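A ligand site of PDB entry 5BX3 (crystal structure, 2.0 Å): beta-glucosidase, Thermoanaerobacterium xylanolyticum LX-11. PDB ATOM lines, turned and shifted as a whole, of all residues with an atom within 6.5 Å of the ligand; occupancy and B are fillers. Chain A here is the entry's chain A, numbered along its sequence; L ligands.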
ATOM      1  N   GLU A 426      30.217  -8.033 -13.783  1.00  0.00           N
ATOM      2  CA  GLU A 426      28.817  -7.723 -13.526  1.00  0.00           C
ATOM      3  C   GLU A 426      28.433  -6.476 -14.317  1.00  0.00           C
ATOM      4  O   GLU A 426      27.413  -6.443 -14.987  1.00  0.00           O
ATOM      5  CB  GLU A 426      28.586  -7.534 -12.027  1.00  0.00           C
ATOM      6  CG  GLU A 426      27.195  -7.103 -11.649  1.00  0.00           C
ATOM      7  CD  GLU A 426      27.041  -6.759 -10.194  1.00  0.00           C
ATOM      8  OE1 GLU A 426      27.862  -7.210  -9.360  1.00  0.00           O
ATOM      9  OE2 GLU A 426      26.052  -6.061  -9.895  1.00  0.00           O
ATOM     10  N   TYR A 430      29.717  -1.381 -10.955  1.00  0.00           N
ATOM     11  CA  TYR A 430      29.891  -2.352  -9.874  1.00  0.00           C
ATOM     12  C   TYR A 430      30.893  -3.374 -10.393  1.00  0.00           C
ATOM     13  O   TYR A 430      30.526  -4.436 -10.963  1.00  0.00           O
ATOM     14  CB  TYR A 430      28.560  -3.027  -9.506  1.00  0.00           C
ATOM     15  CG  TYR A 430      27.367  -2.109  -9.420  1.00  0.00           C
ATOM     16  CD1 TYR A 430      27.451  -0.829  -8.873  1.00  0.00           C
ATOM     17  CD2 TYR A 430      26.106  -2.552  -9.843  1.00  0.00           C
ATOM     18  CE1 TYR A 430      26.331   0.001  -8.789  1.00  0.00           C
ATOM     19  CE2 TYR A 430      24.986  -1.745  -9.738  1.00  0.00           C
ATOM     20  CZ  TYR A 430      25.097  -0.473  -9.209  1.00  0.00           C
ATOM     21  OH  TYR A 430      23.977   0.314  -9.134  1.00  0.00           O
ATOM     22  N   TYR A 432      32.841  -6.022 -10.417  1.00  0.00           N
ATOM     23  CA  TYR A 432      33.005  -7.324  -9.776  1.00  0.00           C
ATOM     24  C   TYR A 432      32.941  -8.448 -10.832  1.00  0.00           C
ATOM     25  O   TYR A 432      32.025  -8.448 -11.654  1.00  0.00           O
ATOM     26  CB  TYR A 432      31.886  -7.541  -8.753  1.00  0.00           C
ATOM     27  CG  TYR A 432      31.763  -6.388  -7.754  1.00  0.00           C
ATOM     28  CD1 TYR A 432      32.859  -5.990  -7.000  1.00  0.00           C
ATOM     29  CD2 TYR A 432      30.569  -5.709  -7.579  1.00  0.00           C
ATOM     30  CE1 TYR A 432      32.765  -4.939  -6.092  1.00  0.00           C
ATOM     31  CE2 TYR A 432      30.464  -4.645  -6.675  1.00  0.00           C
ATOM     32  CZ  TYR A 432      31.570  -4.279  -5.948  1.00  0.00           C
ATOM     33  OH  TYR A 432      31.489  -3.255  -5.036  1.00  0.00           O
ATOM     34  N   THR A 435      29.886 -12.020 -10.651  1.00  0.00           N
ATOM     35  CA  THR A 435      28.944 -11.959  -9.555  1.00  0.00           C
ATOM     36  C   THR A 435      27.927 -13.080  -9.711  1.00  0.00           C
ATOM     37  O   THR A 435      27.164 -13.106 -10.668  1.00  0.00           O
ATOM     38  CB  THR A 435      28.245 -10.623  -9.529  1.00  0.00           C
ATOM     39  OG1 THR A 435      29.255  -9.623  -9.413  1.00  0.00           O
ATOM     40  CG2 THR A 435      27.263 -10.533  -8.367  1.00  0.00           C
ATOM     41  N   ASP A 437      25.144 -14.207  -8.051  1.00  0.00           N
ATOM     42  CA  ASP A 437      23.697 -14.010  -8.001  1.00  0.00           C
ATOM     43  C   ASP A 437      23.169 -13.402  -9.290  1.00  0.00           C
ATOM     44  O   ASP A 437      21.981 -13.526  -9.574  1.00  0.00           O
ATOM     45  CB  ASP A 437      23.295 -13.126  -6.802  1.00  0.00           C
ATOM     46  CG  ASP A 437      24.127 -11.868  -6.705  1.00  0.00           C
ATOM     47  OD1 ASP A 437      25.348 -11.983  -6.412  1.00  0.00           O
ATOM     48  OD2 ASP A 437      23.586 -10.765  -6.907  1.00  0.00           O
ATOM     49  N   VAL A 438      24.044 -12.714 -10.007  1.00  0.00           N
ATOM     50  CA  VAL A 438      23.742 -12.142 -11.327  1.00  0.00           C
ATOM     51  C   VAL A 438      23.980 -13.131 -12.490  1.00  0.00           C
ATOM     52  O   VAL A 438      23.176 -13.186 -13.438  1.00  0.00           O
ATOM     53  CB  VAL A 438      24.620 -10.897 -11.561  1.00  0.00           C
ATOM     54  CG1 VAL A 438      24.385 -10.343 -12.951  1.00  0.00           C
ATOM     55  CG2 VAL A 438      24.341  -9.827 -10.506  1.00  0.00           C
ATOM     56  N   HIS A 492      30.256 -13.965  -3.314  1.00  0.00           N
ATOM     57  CA  HIS A 492      29.523 -13.077  -4.185  1.00  0.00           C
ATOM     58  C   HIS A 492      30.178 -12.891  -5.556  1.00  0.00           C
ATOM     59  O   HIS A 492      29.489 -12.833  -6.574  1.00  0.00           O
ATOM     60  CB  HIS A 492      29.365 -11.729  -3.505  1.00  0.00           C
ATOM     61  CG  HIS A 492      28.700 -10.693  -4.357  1.00  0.00           C
ATOM     62  ND1 HIS A 492      29.418  -9.813  -5.128  1.00  0.00           N
ATOM     63  CD2 HIS A 492      27.406 -10.372  -4.516  1.00  0.00           C
ATOM     64  CE1 HIS A 492      28.582  -8.981  -5.732  1.00  0.00           C
ATOM     65  NE2 HIS A 492      27.352  -9.291  -5.372  1.00  0.00           N
ATOM     66  N   ASP A 493      31.503 -12.803  -5.570  1.00  0.00           N
ATOM     67  CA  ASP A 493      32.242 -12.480  -6.772  1.00  0.00           C
ATOM     68  C   ASP A 493      33.681 -12.962  -6.632  1.00  0.00           C
ATOM     69  O   ASP A 493      34.158 -13.302  -5.535  1.00  0.00           O
ATOM     70  CB  ASP A 493      32.196 -10.958  -7.033  1.00  0.00           C
ATOM     71  CG  ASP A 493      32.870 -10.169  -5.923  1.00  0.00           C
ATOM     72  OD1 ASP A 493      34.124 -10.199  -5.890  1.00  0.00           O
ATOM     73  OD2 ASP A 493      32.135  -9.558  -5.091  1.00  0.00           O
ATOM     74  N   TYR A 508      32.927  -7.122  -3.436  1.00  0.00           N
ATOM     75  CA  TYR A 508      31.691  -6.469  -3.050  1.00  0.00           C
ATOM     76  C   TYR A 508      31.554  -6.294  -1.522  1.00  0.00           C
ATOM     77  O   TYR A 508      31.773  -7.265  -0.772  1.00  0.00           O
ATOM     78  CB  TYR A 508      30.527  -7.328  -3.537  1.00  0.00           C
ATOM     79  CG  TYR A 508      29.144  -6.918  -3.149  1.00  0.00           C
ATOM     80  CD1 TYR A 508      28.436  -5.932  -3.849  1.00  0.00           C
ATOM     81  CD2 TYR A 508      28.492  -7.574  -2.097  1.00  0.00           C
ATOM     82  CE1 TYR A 508      27.118  -5.608  -3.503  1.00  0.00           C
ATOM     83  CE2 TYR A 508      27.196  -7.253  -1.746  1.00  0.00           C
ATOM     84  CZ  TYR A 508      26.514  -6.277  -2.447  1.00  0.00           C
ATOM     85  OH  TYR A 508      25.212  -5.996  -2.064  1.00  0.00           O
ATOM     86  N   TRP A 516      24.101 -14.204   2.665  1.00  0.00           N
ATOM     87  CA  TRP A 516      23.055 -14.217   1.633  1.00  0.00           C
ATOM     88  C   TRP A 516      22.390 -15.577   1.562  1.00  0.00           C
ATOM     89  O   TRP A 516      23.014 -16.598   1.824  1.00  0.00           O
ATOM     90  CB  TRP A 516      23.593 -13.772   0.278  1.00  0.00           C
ATOM     91  CG  TRP A 516      23.712 -12.286   0.188  1.00  0.00           C
ATOM     92  CD1 TRP A 516      23.741 -11.406   1.245  1.00  0.00           C
ATOM     93  CD2 TRP A 516      23.843 -11.483  -0.993  1.00  0.00           C
ATOM     94  NE1 TRP A 516      23.845 -10.123   0.801  1.00  0.00           N
ATOM     95  CE2 TRP A 516      23.905 -10.130  -0.578  1.00  0.00           C
ATOM     96  CE3 TRP A 516      23.869 -11.770  -2.368  1.00  0.00           C
ATOM     97  CZ2 TRP A 516      24.016  -9.087  -1.483  1.00  0.00           C
ATOM     98  CZ3 TRP A 516      23.980 -10.729  -3.256  1.00  0.00           C
ATOM     99  CH2 TRP A 516      24.042  -9.400  -2.820  1.00  0.00           C
ATOM    100  N   GLN A 575      20.315 -10.997  -0.268  1.00  0.00           N
ATOM    101  CA  GLN A 575      20.218 -11.675  -1.551  1.00  0.00           C
ATOM    102  C   GLN A 575      20.371 -10.628  -2.664  1.00  0.00           C
ATOM    103  O   GLN A 575      20.596  -9.457  -2.392  1.00  0.00           O
ATOM    104  CB  GLN A 575      18.909 -12.506  -1.660  1.00  0.00           C
ATOM    105  CG  GLN A 575      17.671 -11.900  -0.993  1.00  0.00           C
ATOM    106  CD  GLN A 575      17.304 -10.540  -1.554  1.00  0.00           C
ATOM    107  OE1 GLN A 575      17.170 -10.387  -2.765  1.00  0.00           O
ATOM    108  NE2 GLN A 575      17.105  -9.570  -0.677  1.00  0.00           N
ATOM    109  N   THR A 576      20.226 -11.065  -3.920  1.00  0.00           N
ATOM    110  CA  THR A 576      20.525 -10.231  -5.097  1.00  0.00           C
ATOM    111  C   THR A 576      19.830  -8.880  -5.162  1.00  0.00           C
ATOM    112  O   THR A 576      20.380  -7.899  -5.688  1.00  0.00           O
ATOM    113  CB  THR A 576      20.269 -11.014  -6.419  1.00  0.00           C
ATOM    114  OG1 THR A 576      20.983 -10.396  -7.497  1.00  0.00           O
ATOM    115  CG2 THR A 576      18.827 -11.071  -6.756  1.00  0.00           C
ATOM    116  N   TYR A 577      18.613  -8.812  -4.642  1.00  0.00           N
ATOM    117  CA  TYR A 577      17.921  -7.530  -4.481  1.00  0.00           C
ATOM    118  C   TYR A 577      18.483  -6.873  -3.232  1.00  0.00           C
ATOM    119  O   TYR A 577      17.876  -6.905  -2.120  1.00  0.00           O
ATOM    120  CB  TYR A 577      16.394  -7.747  -4.392  1.00  0.00           C
ATOM    121  CG  TYR A 577      15.808  -8.409  -5.624  1.00  0.00           C
ATOM    122  CD1 TYR A 577      15.720  -9.793  -5.728  1.00  0.00           C
ATOM    123  CD2 TYR A 577      15.339  -7.652  -6.679  1.00  0.00           C
ATOM    124  CE1 TYR A 577      15.188 -10.397  -6.856  1.00  0.00           C
ATOM    125  CE2 TYR A 577      14.809  -8.246  -7.829  1.00  0.00           C
ATOM    126  CZ  TYR A 577      14.722  -9.611  -7.903  1.00  0.00           C
ATOM    127  OH  TYR A 577      14.195 -10.200  -9.024  1.00  0.00           O
ATOM    128  N   ASP A 578      19.657  -6.272  -3.411  1.00  0.00           N
ATOM    129  CA  ASP A 578      20.510  -5.906  -2.290  1.00  0.00           C
ATOM    130  C   ASP A 578      20.164  -4.579  -1.591  1.00  0.00           C
ATOM    131  O   ASP A 578      20.914  -4.143  -0.732  1.00  0.00           O
ATOM    132  CB  ASP A 578      22.002  -5.994  -2.673  1.00  0.00           C
ATOM    133  CG  ASP A 578      22.435  -4.907  -3.665  1.00  0.00           C
ATOM    134  OD1 ASP A 578      21.575  -4.189  -4.169  1.00  0.00           O
ATOM    135  OD2 ASP A 578      23.651  -4.809  -3.939  1.00  0.00           O
ATOM    136  N   THR A 579      19.037  -3.965  -1.937  1.00  0.00           N
ATOM    137  CA  THR A 579      18.414  -2.963  -1.065  1.00  0.00           C
ATOM    138  C   THR A 579      16.985  -3.303  -0.685  1.00  0.00           C
ATOM    139  O   THR A 579      16.343  -2.549   0.015  1.00  0.00           O
ATOM    140  CB  THR A 579      18.497  -1.521  -1.640  1.00  0.00           C
ATOM    141  OG1 THR A 579      17.878  -1.457  -2.924  1.00  0.00           O
ATOM    142  CG2 THR A 579      19.925  -1.096  -1.763  1.00  0.00           C
ATOM    143  N   GLN A 712      14.231  -0.726  -5.523  1.00  0.00           N
ATOM    144  CA  GLN A 712      14.315  -1.959  -6.355  1.00  0.00           C
ATOM    145  C   GLN A 712      12.953  -2.544  -6.668  1.00  0.00           C
ATOM    146  O   GLN A 712      12.760  -3.130  -7.717  1.00  0.00           O
ATOM    147  CB  GLN A 712      15.239  -3.007  -5.734  1.00  0.00           C
ATOM    148  CG  GLN A 712      16.702  -2.558  -5.722  1.00  0.00           C
ATOM    149  CD  GLN A 712      17.645  -3.535  -5.054  1.00  0.00           C
ATOM    150  OE1 GLN A 712      17.230  -4.391  -4.274  1.00  0.00           O
ATOM    151  NE2 GLN A 712      18.923  -3.389  -5.336  1.00  0.00           N
ATOM    152  N   GLU A 715      11.623  -0.837  -9.748  1.00  0.00           N
ATOM    153  CA  GLU A 715      12.444  -0.975 -10.938  1.00  0.00           C
ATOM    154  C   GLU A 715      11.991  -2.198 -11.755  1.00  0.00           C
ATOM    155  O   GLU A 715      11.523  -3.202 -11.202  1.00  0.00           O
ATOM    156  CB  GLU A 715      13.921  -1.161 -10.558  1.00  0.00           C
ATOM    157  CG  GLU A 715      14.625   0.090 -10.051  1.00  0.00           C
ATOM    158  CD  GLU A 715      16.099  -0.147  -9.675  1.00  0.00           C
ATOM    159  OE1 GLU A 715      16.451  -1.249  -9.202  1.00  0.00           O
ATOM    160  OE2 GLU A 715      16.909   0.800  -9.855  1.00  0.00           O
ATOM    161  N   TRP A 717      13.868  -4.956 -13.812  1.00  0.00           N
ATOM    162  CA  TRP A 717      15.212  -5.489 -14.025  1.00  0.00           C
ATOM    163  C   TRP A 717      15.192  -6.221 -15.353  1.00  0.00           C
ATOM    164  O   TRP A 717      14.474  -7.180 -15.516  1.00  0.00           O
ATOM    165  CB  TRP A 717      15.662  -6.408 -12.886  1.00  0.00           C
ATOM    166  CG  TRP A 717      16.106  -5.661 -11.676  1.00  0.00           C
ATOM    167  CD1 TRP A 717      15.831  -4.336 -11.394  1.00  0.00           C
ATOM    168  CD2 TRP A 717      16.842  -6.160 -10.551  1.00  0.00           C
ATOM    169  NE1 TRP A 717      16.378  -3.988 -10.195  1.00  0.00           N
ATOM    170  CE2 TRP A 717      16.997  -5.086  -9.645  1.00  0.00           C
ATOM    171  CE3 TRP A 717      17.391  -7.417 -10.218  1.00  0.00           C
ATOM    172  CZ2 TRP A 717      17.688  -5.218  -8.430  1.00  0.00           C
ATOM    173  CZ3 TRP A 717      18.092  -7.540  -9.002  1.00  0.00           C
ATOM    174  CH2 TRP A 717      18.215  -6.448  -8.123  1.00  0.00           C
ATOM    175  N   GLU A 762      21.033  -2.715 -15.912  1.00  0.00           N
ATOM    176  CA  GLU A 762      20.342  -3.537 -14.933  1.00  0.00           C
ATOM    177  C   GLU A 762      18.836  -3.191 -14.894  1.00  0.00           C
ATOM    178  O   GLU A 762      17.996  -4.075 -15.005  1.00  0.00           O
ATOM    179  CB  GLU A 762      20.945  -3.339 -13.550  1.00  0.00           C
ATOM    180  CG  GLU A 762      20.148  -3.824 -12.345  1.00  0.00           C
ATOM    181  CD  GLU A 762      20.365  -5.291 -12.021  1.00  0.00           C
ATOM    182  OE1 GLU A 762      20.028  -6.142 -12.885  1.00  0.00           O
ATOM    183  OE2 GLU A 762      20.880  -5.592 -10.897  1.00  0.00           O
ATOM    184  N   ARG A 771      19.611   2.494 -14.062  1.00  0.00           N
ATOM    185  CA  ARG A 771      20.697   2.184 -13.150  1.00  0.00           C
ATOM    186  C   ARG A 771      21.578   1.107 -13.784  1.00  0.00           C
ATOM    187  O   ARG A 771      21.065   0.048 -14.192  1.00  0.00           O
ATOM    188  CB  ARG A 771      20.153   1.704 -11.815  1.00  0.00           C
ATOM    189  CG  ARG A 771      21.244   1.486 -10.774  1.00  0.00           C
ATOM    190  CD  ARG A 771      20.648   1.382  -9.395  1.00  0.00           C
ATOM    191  NE  ARG A 771      19.724   0.248  -9.285  1.00  0.00           N
ATOM    192  CZ  ARG A 771      20.105  -1.007  -9.080  1.00  0.00           C
ATOM    193  NH1 ARG A 771      21.394  -1.317  -8.984  1.00  0.00           N
ATOM    194  NH2 ARG A 771      19.188  -1.952  -8.976  1.00  0.00           N
ATOM    195  N   ALA A 772      22.873   1.435 -13.881  1.00  0.00           N
ATOM    196  CA  ALA A 772      23.996   0.548 -14.214  1.00  0.00           C
ATOM    197  C   ALA A 772      23.937   0.048 -15.643  1.00  0.00           C
ATOM    198  O   ALA A 772      23.538  -1.084 -15.889  1.00  0.00           O
ATOM    199  CB  ALA A 772      24.113  -0.598 -13.230  1.00  0.00           C
ATOM    200  N   TYR A 775      25.358  -4.071 -18.424  1.00  0.00           N
ATOM    201  CA  TYR A 775      25.106  -4.997 -17.330  1.00  0.00           C
ATOM    202  C   TYR A 775      24.993  -6.446 -17.811  1.00  0.00           C
ATOM    203  O   TYR A 775      24.475  -6.699 -18.879  1.00  0.00           O
ATOM    204  CB  TYR A 775      23.818  -4.557 -16.586  1.00  0.00           C
ATOM    205  CG  TYR A 775      23.822  -5.005 -15.153  1.00  0.00           C
ATOM    206  CD1 TYR A 775      24.572  -4.327 -14.179  1.00  0.00           C
ATOM    207  CD2 TYR A 775      23.076  -6.104 -14.749  1.00  0.00           C
ATOM    208  CE1 TYR A 775      24.591  -4.747 -12.871  1.00  0.00           C
ATOM    209  CE2 TYR A 775      23.112  -6.556 -13.444  1.00  0.00           C
ATOM    210  CZ  TYR A 775      23.850  -5.871 -12.504  1.00  0.00           C
ATOM    211  OH  TYR A 775      23.878  -6.323 -11.222  1.00  0.00           O
ATOM    212  N   ARG A 777      23.252  -9.081 -16.480  1.00  0.00           N
ATOM    213  CA  ARG A 777      22.022  -9.820 -16.239  1.00  0.00           C
ATOM    214  C   ARG A 777      21.134 -10.024 -17.473  1.00  0.00           C
ATOM    215  O   ARG A 777      20.602 -11.116 -17.629  1.00  0.00           O
ATOM    216  CB  ARG A 777      21.207  -9.223 -15.078  1.00  0.00           C
ATOM    217  CG  ARG A 777      20.478 -10.283 -14.265  1.00  0.00           C
ATOM    218  CD  ARG A 777      19.546  -9.690 -13.216  1.00  0.00           C
ATOM    219  NE  ARG A 777      20.203  -8.836 -12.227  1.00  0.00           N
ATOM    220  CZ  ARG A 777      20.605  -9.186 -11.010  1.00  0.00           C
ATOM    221  NH1 ARG A 777      20.442 -10.424 -10.545  1.00  0.00           N
ATOM    222  NH2 ARG A 777      21.159  -8.269 -10.214  1.00  0.00           N
HETATM  223  C1  LIG L   1      25.342  -4.931  -7.186  1.00  0.00           C
HETATM  224  C2  LIG L   1      25.644  -6.304  -6.604  1.00  0.00           C
HETATM  225  O1  LIG L   1      27.018  -6.643  -6.921  1.00  0.00           O
HETATM  226  C3  LIG L   1      24.667  -7.400  -7.052  1.00  0.00           C
HETATM  227  O2  LIG L   1      24.824  -8.584  -6.286  1.00  0.00           O
HETATM  228  C4  LIG L   1      23.202  -6.966  -6.947  1.00  0.00           C
HETATM  229  O3  LIG L   1      22.343  -7.976  -7.469  1.00  0.00           O
HETATM  230  C5  LIG L   1      22.992  -5.675  -7.710  1.00  0.00           C
HETATM  231  N1  LIG L   1      23.907  -4.679  -7.160  1.00  0.00           N
HETATM  232  C6  LIG L   1      21.558  -5.192  -7.688  1.00  0.00           C
HETATM  233  O4  LIG L   1      21.424  -4.118  -8.638  1.00  0.00           O
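CD2 of Tyr 430 touches C1 of the ligand (3.6 Å).
CD2 of Tyr 432 touches O1 of the ligand, at 3.7 Å.
Thr 435 touches the ligand (CG2 to O2, 3.8 Å).
CD1 of Tyr 508 touches O1 of the ligand, at 3.5 Å.
CH2 of Trp 516 touches O2 of the ligand, at 3.6 Å.
Gln 712 touches the ligand.
CH2 of Trp 717 touches C6 of the ligand, 3.6 Å away.
Tyr 775 touches the ligand (OH to C5, 3.7 Å).
Hydrophobic or aromatic side chains within 4 Å of the ligand: Tyr 430, Tyr 432, His 492, Tyr 508, Trp 516 and Trp 717.
Of the 23 residues printed, 16 come within 4 Å of the ligand.
The backbone carbonyl oxygen of Arg 771 sits at hydrogen-bond distance from the backbone NH of Glu 762.
OG1 of Thr 576 lies within hydrogen-bond range of NH1 of Arg 777 (3.1 Å).
The backbone NH (N) of Tyr 508 sits at hydrogen-bond distance from the side-chain carboxylate (OD2) of Asp 493.
O of Tyr 432 lies within hydrogen-bond range of N of Glu 426 (2.8 Å).
A ring nitrogen (ND1) of His 492 is in hydrogen-bond range of the side-chain carboxylate (OD2) of Asp 493.
The side-chain amide oxygen (OE1) of Gln 712 lies within hydrogen-bond range of the backbone NH (N) of Thr 579.
The guanidinium group of Arg 771 is in salt-bridge range of the side-chain carboxylate of Glu 715, 2.8 Å away.
OH of Tyr 775 is in hydrogen-bond range of OE2 of Glu 426, at 2.6 Å.
OD2 of Asp 578 lies within salt-bridge range of N1 of the ligand (3.2 Å).
An oxygen (O2) of the ligand lies within hydrogen-bond range of the side-chain carboxylate (OD2) of Asp 437.
The guanidinium group of Arg 771 lies within hydrogen-bond range of an oxygen (O4) of the ligand (2.8 Å).
A ring nitrogen (NE2) of His 492 sits at hydrogen-bond distance from an oxygen (O2) of the ligand, 2.8 Å away.
OE2 of Glu 426 is in salt-bridge range of N1 of the ligand, at 3.7 Å.
OG1 of Thr 576 is in hydrogen-bond range of O3 of the ligand, at 2.8 Å.
O3 of the ligand is in hydrogen-bond range of O of Thr 576, at 2.7 Å.
OE2 of Glu 762 is in hydrogen-bond range of O4 of the ligand, at 2.8 Å.
An oxygen (O3) of the ligand sits at hydrogen-bond distance from the guanidinium group (NH2) of Arg 777 (3.0 Å).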
